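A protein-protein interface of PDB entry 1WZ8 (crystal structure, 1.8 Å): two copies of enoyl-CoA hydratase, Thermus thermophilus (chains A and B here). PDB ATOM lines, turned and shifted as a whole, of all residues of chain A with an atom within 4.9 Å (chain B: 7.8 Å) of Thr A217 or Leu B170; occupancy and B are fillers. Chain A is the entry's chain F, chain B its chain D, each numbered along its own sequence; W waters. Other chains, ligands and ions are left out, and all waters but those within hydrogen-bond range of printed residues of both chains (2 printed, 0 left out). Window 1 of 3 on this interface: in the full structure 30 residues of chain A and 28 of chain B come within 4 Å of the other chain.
The side-chain carboxylate (OD1) of Asp A127 is in salt-bridge range of the side-chain amino group (NZ) of Lys B166 (2.8 Å). OG1 of Thr A217 sits at hydrogen-bond distance from N of Ala B148 (3.1 Å). The side-chain amino group (NZ) of Lys B166 lies within hydrogen-bond range of the side-chain amide oxygen (OD1) of Asn A222 (2.6 Å).
NZ of Lys A218 is in salt-bridge range of OD2 of Asp A127, 2.8 Å away. N of Val B146 is in hydrogen-bond range of O of His B141 (3.1 Å). The side-chain amide oxygen of Asn B172 is in hydrogen-bond range of the backbone NH of Leu B142, at 3.5 Å. The backbone carbonyl oxygen (O) of Ala A213 is in hydrogen-bond range of the side-chain hydroxyl (OG1) of Thr A217, at 2.8 Å.
Among the printed residues, pairs that only touch across the chains: Leu A206 with Leu B170 (3.9 Å), Leu A206 with Leu B171 (3.6 Å), Ala A213 with Leu B142 (3.9 Å), Ala A213 with Val B146 (3.4 Å), Ala A213 with Ala B147 (3.6 Å), Leu A214 with Leu B142 (3.5 Å), Leu A214 with Leu B170 (3.5 Å), His A216 with Ala B147 (3.98 Å), Thr A217 with Leu B142 (3.7 Å), Thr A217 with Ala B147 (3.3 Å), Thr A217 with Leu B170 (3.8 Å), Ala A220 with Val B153 (3.7 Å), Ala A220 with Ser B235 (3.7 Å), Leu A221 with Val B153 (3.9 Å), Leu A221 with Met B162 (3.6 Å) and Leu A221 with Leu B169 (3.9 Å).
Of chain B, only Leu B142 (3.7 Å), Ala B147 (3.3 Å), Ala B148 (3.1 Å) and Leu B170 (3.8 Å) come within 4 Å of Thr A217. Printed residues of chain B within 4 Å of Ala A220: Val B153 (3.7 Å) and Ser B235 (3.7 Å). Printed residues of chain A within 4 Å of Val B153: Ala A220 and Leu A221. Printed residues of chain A within 4 Å of Met B162: Leu A221. Of chain A, only Leu A206, Leu A214 and Thr A217 come within 4 Å of Leu B170. Of the printed residues of chain A, Leu B171 touches Leu A206 (3.6 Å). Printed residues of chain A within 4 Å of Ser B235: Ala A220 (3.7 Å).
Of the 12 printed residues of chain A, 9 touch a printed residue of chain B. Printed residues of chain A that touch a printed residue of chain B: Asp A127, Leu A206, Ala A213, Leu A214, His A216, Thr A217, Ala A220, Leu A221 and Asn A222. Hydrophobic or aromatic side chains of chain A that line the printed part of chain B: Leu A206, Ala A213, Leu A214, His A216, Ala A220 and Leu A221. Along chain B the printed residues that touch a printed residue of chain A span positions 142 to 235. Among the printed residues, 19 pairs touch across the chains.
No position is printed for both chains. Of the 19 pairs that touch across the chains among the printed residues, none has its exchanged pair printed and touching as well.
Water W1 lies within hydrogen-bond range of the side-chain carboxylate (OD1) of Asp A127, the side-chain amino group (NZ) of Lys B166 and the side-chain amide nitrogen (ND2) of Asn A222. Water W2 bridges the backbone carbonyl oxygen of Ala B163 (2.6 Å) and the backbone carbonyl oxygen of Asp A127 (2.8 Å).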
ATOM      1  N   ASP A 127      -7.889   4.098  -2.169  1.00  0.00           N
ATOM      2  CA  ASP A 127      -7.141   4.773  -3.224  1.00  0.00           C
ATOM      3  C   ASP A 127      -5.800   5.285  -2.728  1.00  0.00           C
ATOM      4  O   ASP A 127      -4.790   5.162  -3.419  1.00  0.00           O
ATOM      5  CB  ASP A 127      -7.969   5.915  -3.786  1.00  0.00           C
ATOM      6  CG  ASP A 127      -9.241   5.423  -4.427  1.00  0.00           C
ATOM      7  OD1 ASP A 127      -9.145   4.755  -5.483  1.00  0.00           O
ATOM      8  OD2 ASP A 127     -10.327   5.684  -3.865  1.00  0.00           O
ATOM      9  N   LEU A 206      -8.660  16.007  -1.265  1.00  0.00           N
ATOM     10  CA  LEU A 206      -9.461  15.328  -2.277  1.00  0.00           C
ATOM     11  C   LEU A 206     -10.883  15.883  -2.285  1.00  0.00           C
ATOM     12  O   LEU A 206     -11.491  16.036  -3.343  1.00  0.00           O
ATOM     13  CB  LEU A 206      -9.488  13.823  -2.004  1.00  0.00           C
ATOM     14  CG  LEU A 206      -8.150  13.105  -2.221  1.00  0.00           C
ATOM     15  CD1 LEU A 206      -8.160  11.774  -1.486  1.00  0.00           C
ATOM     16  CD2 LEU A 206      -7.906  12.910  -3.716  1.00  0.00           C
ATOM     17  N   ALA A 213     -14.332  14.871 -12.112  1.00  0.00           N
ATOM     18  CA  ALA A 213     -13.016  14.516 -12.634  1.00  0.00           C
ATOM     19  C   ALA A 213     -12.336  13.447 -11.782  1.00  0.00           C
ATOM     20  O   ALA A 213     -11.707  12.538 -12.317  1.00  0.00           O
ATOM     21  CB  ALA A 213     -12.142  15.749 -12.729  1.00  0.00           C
ATOM     22  N   LEU A 214     -12.454  13.566 -10.459  1.00  0.00           N
ATOM     23  CA  LEU A 214     -11.859  12.594  -9.548  1.00  0.00           C
ATOM     24  C   LEU A 214     -12.527  11.235  -9.713  1.00  0.00           C
ATOM     25  O   LEU A 214     -11.858  10.205  -9.734  1.00  0.00           O
ATOM     26  CB  LEU A 214     -11.994  13.077  -8.099  1.00  0.00           C
ATOM     27  CG  LEU A 214     -10.973  14.145  -7.691  1.00  0.00           C
ATOM     28  CD1 LEU A 214     -11.419  14.853  -6.421  1.00  0.00           C
ATOM     29  CD2 LEU A 214      -9.617  13.482  -7.494  1.00  0.00           C
ATOM     30  N   HIS A 215     -13.852  11.244  -9.834  1.00  0.00           N
ATOM     31  CA  HIS A 215     -14.624  10.020 -10.014  1.00  0.00           C
ATOM     32  C   HIS A 215     -14.181   9.303 -11.284  1.00  0.00           C
ATOM     33  O   HIS A 215     -13.877   8.110 -11.259  1.00  0.00           O
ATOM     34  CB  HIS A 215     -16.121  10.358 -10.085  1.00  0.00           C
ATOM     35  CG  HIS A 215     -16.994   9.211 -10.492  1.00  0.00           C
ATOM     36  ND1 HIS A 215     -16.657   7.894 -10.264  1.00  0.00           N
ATOM     37  CD2 HIS A 215     -18.215   9.189 -11.079  1.00  0.00           C
ATOM     38  CE1 HIS A 215     -17.632   7.111 -10.693  1.00  0.00           C
ATOM     39  NE2 HIS A 215     -18.589   7.873 -11.192  1.00  0.00           N
ATOM     40  N   HIS A 216     -14.124  10.043 -12.384  1.00  0.00           N
ATOM     41  CA  HIS A 216     -13.734   9.469 -13.664  1.00  0.00           C
ATOM     42  C   HIS A 216     -12.290   8.988 -13.715  1.00  0.00           C
ATOM     43  O   HIS A 216     -11.995   7.970 -14.336  1.00  0.00           O
ATOM     44  CB  HIS A 216     -14.005  10.479 -14.781  1.00  0.00           C
ATOM     45  CG  HIS A 216     -15.461  10.772 -14.976  1.00  0.00           C
ATOM     46  ND1 HIS A 216     -15.923  11.695 -15.888  1.00  0.00           N
ATOM     47  CD2 HIS A 216     -16.561  10.265 -14.367  1.00  0.00           C
ATOM     48  CE1 HIS A 216     -17.242  11.747 -15.833  1.00  0.00           C
ATOM     49  NE2 HIS A 216     -17.653  10.887 -14.917  1.00  0.00           N
ATOM     50  N   THR A 217     -11.388   9.706 -13.060  1.00  0.00           N
ATOM     51  CA  THR A 217      -9.987   9.297 -13.070  1.00  0.00           C
ATOM     52  C   THR A 217      -9.834   8.026 -12.237  1.00  0.00           C
ATOM     53  O   THR A 217      -9.158   7.078 -12.653  1.00  0.00           O
ATOM     54  CB  THR A 217      -9.092  10.411 -12.511  1.00  0.00           C
ATOM     55  OG1 THR A 217      -9.275  11.601 -13.289  1.00  0.00           O
ATOM     56  CG2 THR A 217      -7.628  10.002 -12.565  1.00  0.00           C
ATOM     57  N   LYS A 218     -10.466   7.998 -11.066  1.00  0.00           N
ATOM     58  CA  LYS A 218     -10.396   6.816 -10.215  1.00  0.00           C
ATOM     59  C   LYS A 218     -11.011   5.638 -10.952  1.00  0.00           C
ATOM     60  O   LYS A 218     -10.451   4.539 -10.979  1.00  0.00           O
ATOM     61  CB  LYS A 218     -11.163   7.029  -8.903  1.00  0.00           C
ATOM     62  CG  LYS A 218     -11.381   5.732  -8.115  1.00  0.00           C
ATOM     63  CD  LYS A 218     -12.105   5.966  -6.793  1.00  0.00           C
ATOM     64  CE  LYS A 218     -12.384   4.642  -6.097  1.00  0.00           C
ATOM     65  NZ  LYS A 218     -12.867   4.816  -4.706  1.00  0.00           N
ATOM     66  N   HIS A 219     -12.171   5.872 -11.551  1.00  0.00           N
ATOM     67  CA  HIS A 219     -12.857   4.812 -12.278  1.00  0.00           C
ATOM     68  C   HIS A 219     -11.992   4.256 -13.403  1.00  0.00           C
ATOM     69  O   HIS A 219     -11.857   3.038 -13.548  1.00  0.00           O
ATOM     70  CB  HIS A 219     -14.162   5.340 -12.868  1.00  0.00           C
ATOM     71  CG  HIS A 219     -14.950   4.296 -13.596  1.00  0.00           C
ATOM     72  ND1 HIS A 219     -15.706   3.346 -12.944  1.00  0.00           N
ATOM     73  CD2 HIS A 219     -15.053   4.019 -14.918  1.00  0.00           C
ATOM     74  CE1 HIS A 219     -16.241   2.526 -13.834  1.00  0.00           C
ATOM     75  NE2 HIS A 219     -15.859   2.913 -15.039  1.00  0.00           N
ATOM     76  N   ALA A 220     -11.395   5.152 -14.187  1.00  0.00           N
ATOM     77  CA  ALA A 220     -10.571   4.740 -15.323  1.00  0.00           C
ATOM     78  C   ALA A 220      -9.333   3.987 -14.867  1.00  0.00           C
ATOM     79  O   ALA A 220      -8.957   2.978 -15.463  1.00  0.00           O
ATOM     80  CB  ALA A 220     -10.167   5.953 -16.146  1.00  0.00           C
ATOM     81  N   LEU A 221      -8.685   4.488 -13.822  1.00  0.00           N
ATOM     82  CA  LEU A 221      -7.495   3.827 -13.306  1.00  0.00           C
ATOM     83  C   LEU A 221      -7.830   2.436 -12.768  1.00  0.00           C
ATOM     84  O   LEU A 221      -7.086   1.484 -12.996  1.00  0.00           O
ATOM     85  CB  LEU A 221      -6.855   4.667 -12.193  1.00  0.00           C
ATOM     86  CG  LEU A 221      -5.996   5.852 -12.645  1.00  0.00           C
ATOM     87  CD1 LEU A 221      -5.541   6.667 -11.443  1.00  0.00           C
ATOM     88  CD2 LEU A 221      -4.788   5.322 -13.400  1.00  0.00           C
ATOM     89  N   ASN A 222      -8.962   2.318 -12.076  1.00  0.00           N
ATOM     90  CA  ASN A 222      -9.348   1.040 -11.498  1.00  0.00           C
ATOM     91  C   ASN A 222      -9.674  -0.074 -12.486  1.00  0.00           C
ATOM     92  O   ASN A 222      -9.761  -1.238 -12.092  1.00  0.00           O
ATOM     93  CB  ASN A 222     -10.489   1.232 -10.491  1.00  0.00           C
ATOM     94  CG  ASN A 222      -9.983   1.723  -9.144  1.00  0.00           C
ATOM     95  OD1 ASN A 222      -8.773   1.718  -8.890  1.00  0.00           O
ATOM     96  ND2 ASN A 222     -10.900   2.136  -8.270  1.00  0.00           N
ATOM     97  N   ASP B 139       0.965  15.784 -13.942  1.00  0.00           N
ATOM     98  CA  ASP B 139      -0.106  15.456 -14.878  1.00  0.00           C
ATOM     99  C   ASP B 139      -0.892  16.753 -15.065  1.00  0.00           C
ATOM    100  O   ASP B 139      -1.079  17.236 -16.187  1.00  0.00           O
ATOM    101  CB  ASP B 139      -1.018  14.378 -14.290  1.00  0.00           C
ATOM    102  CG  ASP B 139      -2.214  14.104 -15.161  1.00  0.00           C
ATOM    103  OD1 ASP B 139      -2.043  13.452 -16.215  1.00  0.00           O
ATOM    104  OD2 ASP B 139      -3.326  14.556 -14.804  1.00  0.00           O
ATOM    105  N   HIS B 141      -4.177  17.613 -14.781  1.00  0.00           N
ATOM    106  CA  HIS B 141      -5.597  17.669 -15.193  1.00  0.00           C
ATOM    107  C   HIS B 141      -6.588  17.970 -14.039  1.00  0.00           C
ATOM    108  O   HIS B 141      -7.523  18.748 -14.176  1.00  0.00           O
ATOM    109  CB  HIS B 141      -5.955  16.335 -15.849  1.00  0.00           C
ATOM    110  CG  HIS B 141      -5.175  16.177 -17.127  1.00  0.00           C
ATOM    111  ND1 HIS B 141      -4.072  15.394 -17.235  1.00  0.00           N
ATOM    112  CD2 HIS B 141      -5.427  16.762 -18.373  1.00  0.00           C
ATOM    113  CE1 HIS B 141      -3.673  15.505 -18.518  1.00  0.00           C
ATOM    114  NE2 HIS B 141      -4.466  16.317 -19.221  1.00  0.00           N
ATOM    115  N   LEU B 142      -6.404  17.340 -12.884  1.00  0.00           N
ATOM    116  CA  LEU B 142      -7.318  17.529 -11.764  1.00  0.00           C
ATOM    117  C   LEU B 142      -7.356  18.966 -11.246  1.00  0.00           C
ATOM    118  O   LEU B 142      -8.373  19.419 -10.721  1.00  0.00           O
ATOM    119  CB  LEU B 142      -6.967  16.545 -10.641  1.00  0.00           C
ATOM    120  CG  LEU B 142      -7.532  15.120 -10.798  1.00  0.00           C
ATOM    121  CD1 LEU B 142      -9.024  15.143 -10.481  1.00  0.00           C
ATOM    122  CD2 LEU B 142      -7.292  14.578 -12.221  1.00  0.00           C
ATOM    123  N   ARG B 143      -6.248  19.683 -11.407  1.00  0.00           N
ATOM    124  CA  ARG B 143      -6.168  21.074 -10.983  1.00  0.00           C
ATOM    125  C   ARG B 143      -6.950  21.910 -11.996  1.00  0.00           C
ATOM    126  O   ARG B 143      -7.525  22.959 -11.676  1.00  0.00           O
ATOM    127  CB  ARG B 143      -4.710  21.521 -10.965  1.00  0.00           C
ATOM    128  CG  ARG B 143      -4.535  22.937 -10.483  1.00  0.00           C
ATOM    129  CD  ARG B 143      -3.632  23.022  -9.271  1.00  0.00           C
ATOM    130  NE  ARG B 143      -4.430  23.274  -8.076  1.00  0.00           N
ATOM    131  CZ  ARG B 143      -4.821  24.470  -7.645  1.00  0.00           C
ATOM    132  NH1 ARG B 143      -4.484  25.584  -8.292  1.00  0.00           N
ATOM    133  NH2 ARG B 143      -5.590  24.544  -6.567  1.00  0.00           N
ATOM    134  N   VAL B 146     -10.540  18.477 -14.967  1.00  0.00           N
ATOM    135  CA  VAL B 146     -10.934  17.375 -15.837  1.00  0.00           C
ATOM    136  C   VAL B 146     -10.147  16.117 -15.478  1.00  0.00           C
ATOM    137  O   VAL B 146      -9.118  16.183 -14.790  1.00  0.00           O
ATOM    138  CB  VAL B 146     -10.697  17.705 -17.333  1.00  0.00           C
ATOM    139  CG1 VAL B 146     -11.581  18.878 -17.758  1.00  0.00           C
ATOM    140  CG2 VAL B 146      -9.234  18.027 -17.569  1.00  0.00           C
ATOM    141  N   ALA B 147     -10.633  14.974 -15.949  1.00  0.00           N
ATOM    142  CA  ALA B 147      -9.986  13.706 -15.661  1.00  0.00           C
ATOM    143  C   ALA B 147      -8.615  13.597 -16.309  1.00  0.00           C
ATOM    144  O   ALA B 147      -8.338  14.239 -17.326  1.00  0.00           O
ATOM    145  CB  ALA B 147     -10.877  12.551 -16.111  1.00  0.00           C
ATOM    146  N   ALA B 148      -7.756  12.778 -15.713  1.00  0.00           N
ATOM    147  CA  ALA B 148      -6.404  12.574 -16.226  1.00  0.00           C
ATOM    148  C   ALA B 148      -6.491  11.588 -17.389  1.00  0.00           C
ATOM    149  O   ALA B 148      -6.111  10.424 -17.257  1.00  0.00           O
ATOM    150  CB  ALA B 148      -5.527  12.018 -15.130  1.00  0.00           C
ATOM    151  N   GLY B 149      -6.976  12.059 -18.534  1.00  0.00           N
ATOM    152  CA  GLY B 149      -7.142  11.158 -19.657  1.00  0.00           C
ATOM    153  C   GLY B 149      -6.262  11.267 -20.882  1.00  0.00           C
ATOM    154  O   GLY B 149      -6.541  10.578 -21.869  1.00  0.00           O
ATOM    155  N   ALA B 152      -1.959   9.361 -18.626  1.00  0.00           N
ATOM    156  CA  ALA B 152      -1.801   8.731 -17.321  1.00  0.00           C
ATOM    157  C   ALA B 152      -2.379   7.336 -17.121  1.00  0.00           C
ATOM    158  O   ALA B 152      -1.761   6.500 -16.457  1.00  0.00           O
ATOM    159  CB  ALA B 152      -2.329   9.667 -16.238  1.00  0.00           C
ATOM    160  N   VAL B 153      -3.558   7.076 -17.673  1.00  0.00           N
ATOM    161  CA  VAL B 153      -4.175   5.769 -17.496  1.00  0.00           C
ATOM    162  C   VAL B 153      -3.557   4.709 -18.394  1.00  0.00           C
ATOM    163  O   VAL B 153      -3.710   3.517 -18.142  1.00  0.00           O
ATOM    164  CB  VAL B 153      -5.704   5.846 -17.724  1.00  0.00           C
ATOM    165  CG1 VAL B 153      -6.328   4.454 -17.667  1.00  0.00           C
ATOM    166  CG2 VAL B 153      -6.319   6.733 -16.660  1.00  0.00           C
ATOM    167  N   MET B 162       0.160   1.373  -9.042  1.00  0.00           N
ATOM    168  CA  MET B 162      -1.107   2.059  -8.793  1.00  0.00           C
ATOM    169  C   MET B 162      -1.161   2.998  -7.595  1.00  0.00           C
ATOM    170  O   MET B 162      -1.891   3.984  -7.630  1.00  0.00           O
ATOM    171  CB  MET B 162      -2.236   1.039  -8.664  1.00  0.00           C
ATOM    172  CG  MET B 162      -3.625   1.657  -8.768  1.00  0.00           C
ATOM    173  SD  MET B 162      -3.822   2.506 -10.360  1.00  0.00           S
ATOM    174  CE  MET B 162      -3.882   1.110 -11.464  1.00  0.00           C
ATOM    175  N   ALA B 163      -0.408   2.697  -6.538  1.00  0.00           N
ATOM    176  CA  ALA B 163      -0.413   3.546  -5.347  1.00  0.00           C
ATOM    177  C   ALA B 163       0.200   4.913  -5.642  1.00  0.00           C
ATOM    178  O   ALA B 163      -0.377   5.954  -5.316  1.00  0.00           O
ATOM    179  CB  ALA B 163       0.351   2.863  -4.206  1.00  0.00           C
ATOM    180  N   LYS B 164       1.373   4.915  -6.262  1.00  0.00           N
ATOM    181  CA  LYS B 164       2.030   6.168  -6.580  1.00  0.00           C
ATOM    182  C   LYS B 164       1.302   6.890  -7.705  1.00  0.00           C
ATOM    183  O   LYS B 164       1.300   8.119  -7.759  1.00  0.00           O
ATOM    184  CB  LYS B 164       3.497   5.919  -6.946  1.00  0.00           C
ATOM    185  CG  LYS B 164       4.330   5.419  -5.775  1.00  0.00           C
ATOM    186  CD  LYS B 164       4.422   6.456  -4.651  1.00  0.00           C
ATOM    187  CE  LYS B 164       5.218   5.905  -3.467  1.00  0.00           C
ATOM    188  NZ  LYS B 164       5.570   6.974  -2.502  1.00  0.00           N
ATOM    189  N   ALA B 165       0.673   6.130  -8.598  1.00  0.00           N
ATOM    190  CA  ALA B 165      -0.066   6.736  -9.691  1.00  0.00           C
ATOM    191  C   ALA B 165      -1.269   7.493  -9.113  1.00  0.00           C
ATOM    192  O   ALA B 165      -1.464   8.671  -9.404  1.00  0.00           O
ATOM    193  CB  ALA B 165      -0.520   5.660 -10.689  1.00  0.00           C
ATOM    194  N   LYS B 166      -2.060   6.832  -8.275  1.00  0.00           N
ATOM    195  CA  LYS B 166      -3.226   7.486  -7.681  1.00  0.00           C
ATOM    196  C   LYS B 166      -2.875   8.704  -6.827  1.00  0.00           C
ATOM    197  O   LYS B 166      -3.570   9.715  -6.866  1.00  0.00           O
ATOM    198  CB  LYS B 166      -4.020   6.487  -6.844  1.00  0.00           C
ATOM    199  CG  LYS B 166      -4.757   5.467  -7.683  1.00  0.00           C
ATOM    200  CD  LYS B 166      -5.681   4.623  -6.851  1.00  0.00           C
ATOM    201  CE  LYS B 166      -6.586   3.803  -7.751  1.00  0.00           C
ATOM    202  NZ  LYS B 166      -7.541   2.981  -6.972  1.00  0.00           N
ATOM    203  N   TYR B 167      -1.799   8.606  -6.056  1.00  0.00           N
ATOM    204  CA  TYR B 167      -1.380   9.710  -5.202  1.00  0.00           C
ATOM    205  C   TYR B 167      -1.047  10.948  -6.030  1.00  0.00           C
ATOM    206  O   TYR B 167      -1.572  12.035  -5.785  1.00  0.00           O
ATOM    207  CB  TYR B 167      -0.157   9.300  -4.368  1.00  0.00           C
ATOM    208  CG  TYR B 167       0.329  10.365  -3.400  1.00  0.00           C
ATOM    209  CD1 TYR B 167      -0.458  10.763  -2.317  1.00  0.00           C
ATOM    210  CD2 TYR B 167       1.582  10.964  -3.558  1.00  0.00           C
ATOM    211  CE1 TYR B 167      -0.008  11.730  -1.415  1.00  0.00           C
ATOM    212  CE2 TYR B 167       2.041  11.935  -2.657  1.00  0.00           C
ATOM    213  CZ  TYR B 167       1.241  12.311  -1.592  1.00  0.00           C
ATOM    214  OH  TYR B 167       1.680  13.272  -0.702  1.00  0.00           O
ATOM    215  N   HIS B 168      -0.190  10.783  -7.032  1.00  0.00           N
ATOM    216  CA  HIS B 168       0.206  11.923  -7.846  1.00  0.00           C
ATOM    217  C   HIS B 168      -0.834  12.403  -8.842  1.00  0.00           C
ATOM    218  O   HIS B 168      -0.870  13.586  -9.168  1.00  0.00           O
ATOM    219  CB  HIS B 168       1.535  11.615  -8.536  1.00  0.00           C
ATOM    220  CG  HIS B 168       2.676  11.492  -7.575  1.00  0.00           C
ATOM    221  ND1 HIS B 168       3.259  12.586  -6.972  1.00  0.00           N
ATOM    222  CD2 HIS B 168       3.282  10.403  -7.045  1.00  0.00           C
ATOM    223  CE1 HIS B 168       4.174  12.176  -6.112  1.00  0.00           C
ATOM    224  NE2 HIS B 168       4.207  10.856  -6.136  1.00  0.00           N
ATOM    225  N   LEU B 169      -1.695  11.502  -9.303  1.00  0.00           N
ATOM    226  CA  LEU B 169      -2.725  11.862 -10.268  1.00  0.00           C
ATOM    227  C   LEU B 169      -3.954  12.501  -9.639  1.00  0.00           C
ATOM    228  O   LEU B 169      -4.460  13.507 -10.137  1.00  0.00           O
ATOM    229  CB  LEU B 169      -3.153  10.628 -11.060  1.00  0.00           C
ATOM    230  CG  LEU B 169      -2.021  10.030 -11.894  1.00  0.00           C
ATOM    231  CD1 LEU B 169      -2.515   8.784 -12.617  1.00  0.00           C
ATOM    232  CD2 LEU B 169      -1.513  11.066 -12.876  1.00  0.00           C
ATOM    233  N   LEU B 170      -4.426  11.923  -8.541  1.00  0.00           N
ATOM    234  CA  LEU B 170      -5.618  12.439  -7.877  1.00  0.00           C
ATOM    235  C   LEU B 170      -5.381  13.698  -7.044  1.00  0.00           C
ATOM    236  O   LEU B 170      -6.303  14.489  -6.841  1.00  0.00           O
ATOM    237  CB  LEU B 170      -6.230  11.345  -6.994  1.00  0.00           C
ATOM    238  CG  LEU B 170      -6.657  10.049  -7.698  1.00  0.00           C
ATOM    239  CD1 LEU B 170      -7.182   9.065  -6.667  1.00  0.00           C
ATOM    240  CD2 LEU B 170      -7.730  10.352  -8.744  1.00  0.00           C
ATOM    241  N   LEU B 171      -4.155  13.886  -6.558  1.00  0.00           N
ATOM    242  CA  LEU B 171      -3.833  15.056  -5.741  1.00  0.00           C
ATOM    243  C   LEU B 171      -3.097  16.146  -6.507  1.00  0.00           C
ATOM    244  O   LEU B 171      -2.912  17.253  -5.998  1.00  0.00           O
ATOM    245  CB  LEU B 171      -2.979  14.654  -4.538  1.00  0.00           C
ATOM    246  CG  LEU B 171      -3.612  13.814  -3.425  1.00  0.00           C
ATOM    247  CD1 LEU B 171      -2.570  13.581  -2.341  1.00  0.00           C
ATOM    248  CD2 LEU B 171      -4.828  14.526  -2.844  1.00  0.00           C
ATOM    249  N   ASN B 172      -2.670  15.834  -7.721  1.00  0.00           N
ATOM    250  CA  ASN B 172      -1.951  16.805  -8.530  1.00  0.00           C
ATOM    251  C   ASN B 172      -0.675  17.177  -7.782  1.00  0.00           C
ATOM    252  O   ASN B 172      -0.330  18.348  -7.665  1.00  0.00           O
ATOM    253  CB  ASN B 172      -2.821  18.046  -8.747  1.00  0.00           C
ATOM    254  CG  ASN B 172      -2.781  18.548 -10.176  1.00  0.00           C
ATOM    255  OD1 ASN B 172      -3.761  18.447 -10.916  1.00  0.00           O
ATOM    256  ND2 ASN B 172      -1.639  19.095 -10.571  1.00  0.00           N
ATOM    257  N   GLU B 173       0.007  16.160  -7.264  1.00  0.00           N
ATOM    258  CA  GLU B 173       1.251  16.341  -6.523  1.00  0.00           C
ATOM    259  C   GLU B 173       2.447  16.235  -7.472  1.00  0.00           C
ATOM    260  O   GLU B 173       2.764  15.154  -7.979  1.00  0.00           O
ATOM    261  CB  GLU B 173       1.371  15.269  -5.438  1.00  0.00           C
ATOM    262  CG  GLU B 173       2.403  15.573  -4.369  1.00  0.00           C
ATOM    263  CD  GLU B 173       1.901  16.582  -3.355  1.00  0.00           C
ATOM    264  OE1 GLU B 173       1.508  17.692  -3.765  1.00  0.00           O
ATOM    265  OE2 GLU B 173       1.894  16.259  -2.149  1.00  0.00           O
ATOM    266  N   SER B 235     -10.457   6.718 -20.621  1.00  0.00           N
ATOM    267  CA  SER B 235     -10.078   7.829 -19.756  1.00  0.00           C
ATOM    268  C   SER B 235     -10.038   9.114 -20.573  1.00  0.00           C
ATOM    269  O   SER B 235     -10.388  10.185 -20.077  1.00  0.00           O
ATOM    270  CB  SER B 235      -8.711   7.582 -19.102  1.00  0.00           C
ATOM    271  OG  SER B 235      -7.647   7.729 -20.028  1.00  0.00           O
ATOM    272  N   LEU B 238     -13.682  10.160 -21.303  1.00  0.00           N
ATOM    273  CA  LEU B 238     -14.270  10.721 -20.088  1.00  0.00           C
ATOM    274  C   LEU B 238     -13.724  12.114 -19.842  1.00  0.00           C
ATOM    275  O   LEU B 238     -14.459  13.016 -19.426  1.00  0.00           O
ATOM    276  CB  LEU B 238     -13.976   9.827 -18.879  1.00  0.00           C
ATOM    277  CG  LEU B 238     -14.736   8.498 -18.875  1.00  0.00           C
ATOM    278  CD1 LEU B 238     -14.310   7.659 -17.682  1.00  0.00           C
ATOM    279  CD2 LEU B 238     -16.237   8.776 -18.834  1.00  0.00           C
ATOM    280  N   GLU B 239     -12.433  12.299 -20.091  1.00  0.00           N
ATOM    281  CA  GLU B 239     -11.839  13.613 -19.901  1.00  0.00           C
ATOM    282  C   GLU B 239     -12.560  14.621 -20.790  1.00  0.00           C
ATOM    283  O   GLU B 239     -12.989  15.678 -20.330  1.00  0.00           O
ATOM    284  CB  GLU B 239     -10.354  13.619 -20.277  1.00  0.00           C
ATOM    285  CG  GLU B 239      -9.688  14.945 -19.949  1.00  0.00           C
ATOM    286  CD  GLU B 239      -8.330  15.125 -20.592  1.00  0.00           C
ATOM    287  OE1 GLU B 239      -7.610  14.123 -20.775  1.00  0.00           O
ATOM    288  OE2 GLU B 239      -7.973  16.286 -20.896  1.00  0.00           O
HETATM  289  O   HOH W   1      -9.968   2.330  -4.925  1.00  0.00           O
HETATM  290  O   HOH W   2      -2.180   6.040  -3.390  1.00  0.00           O
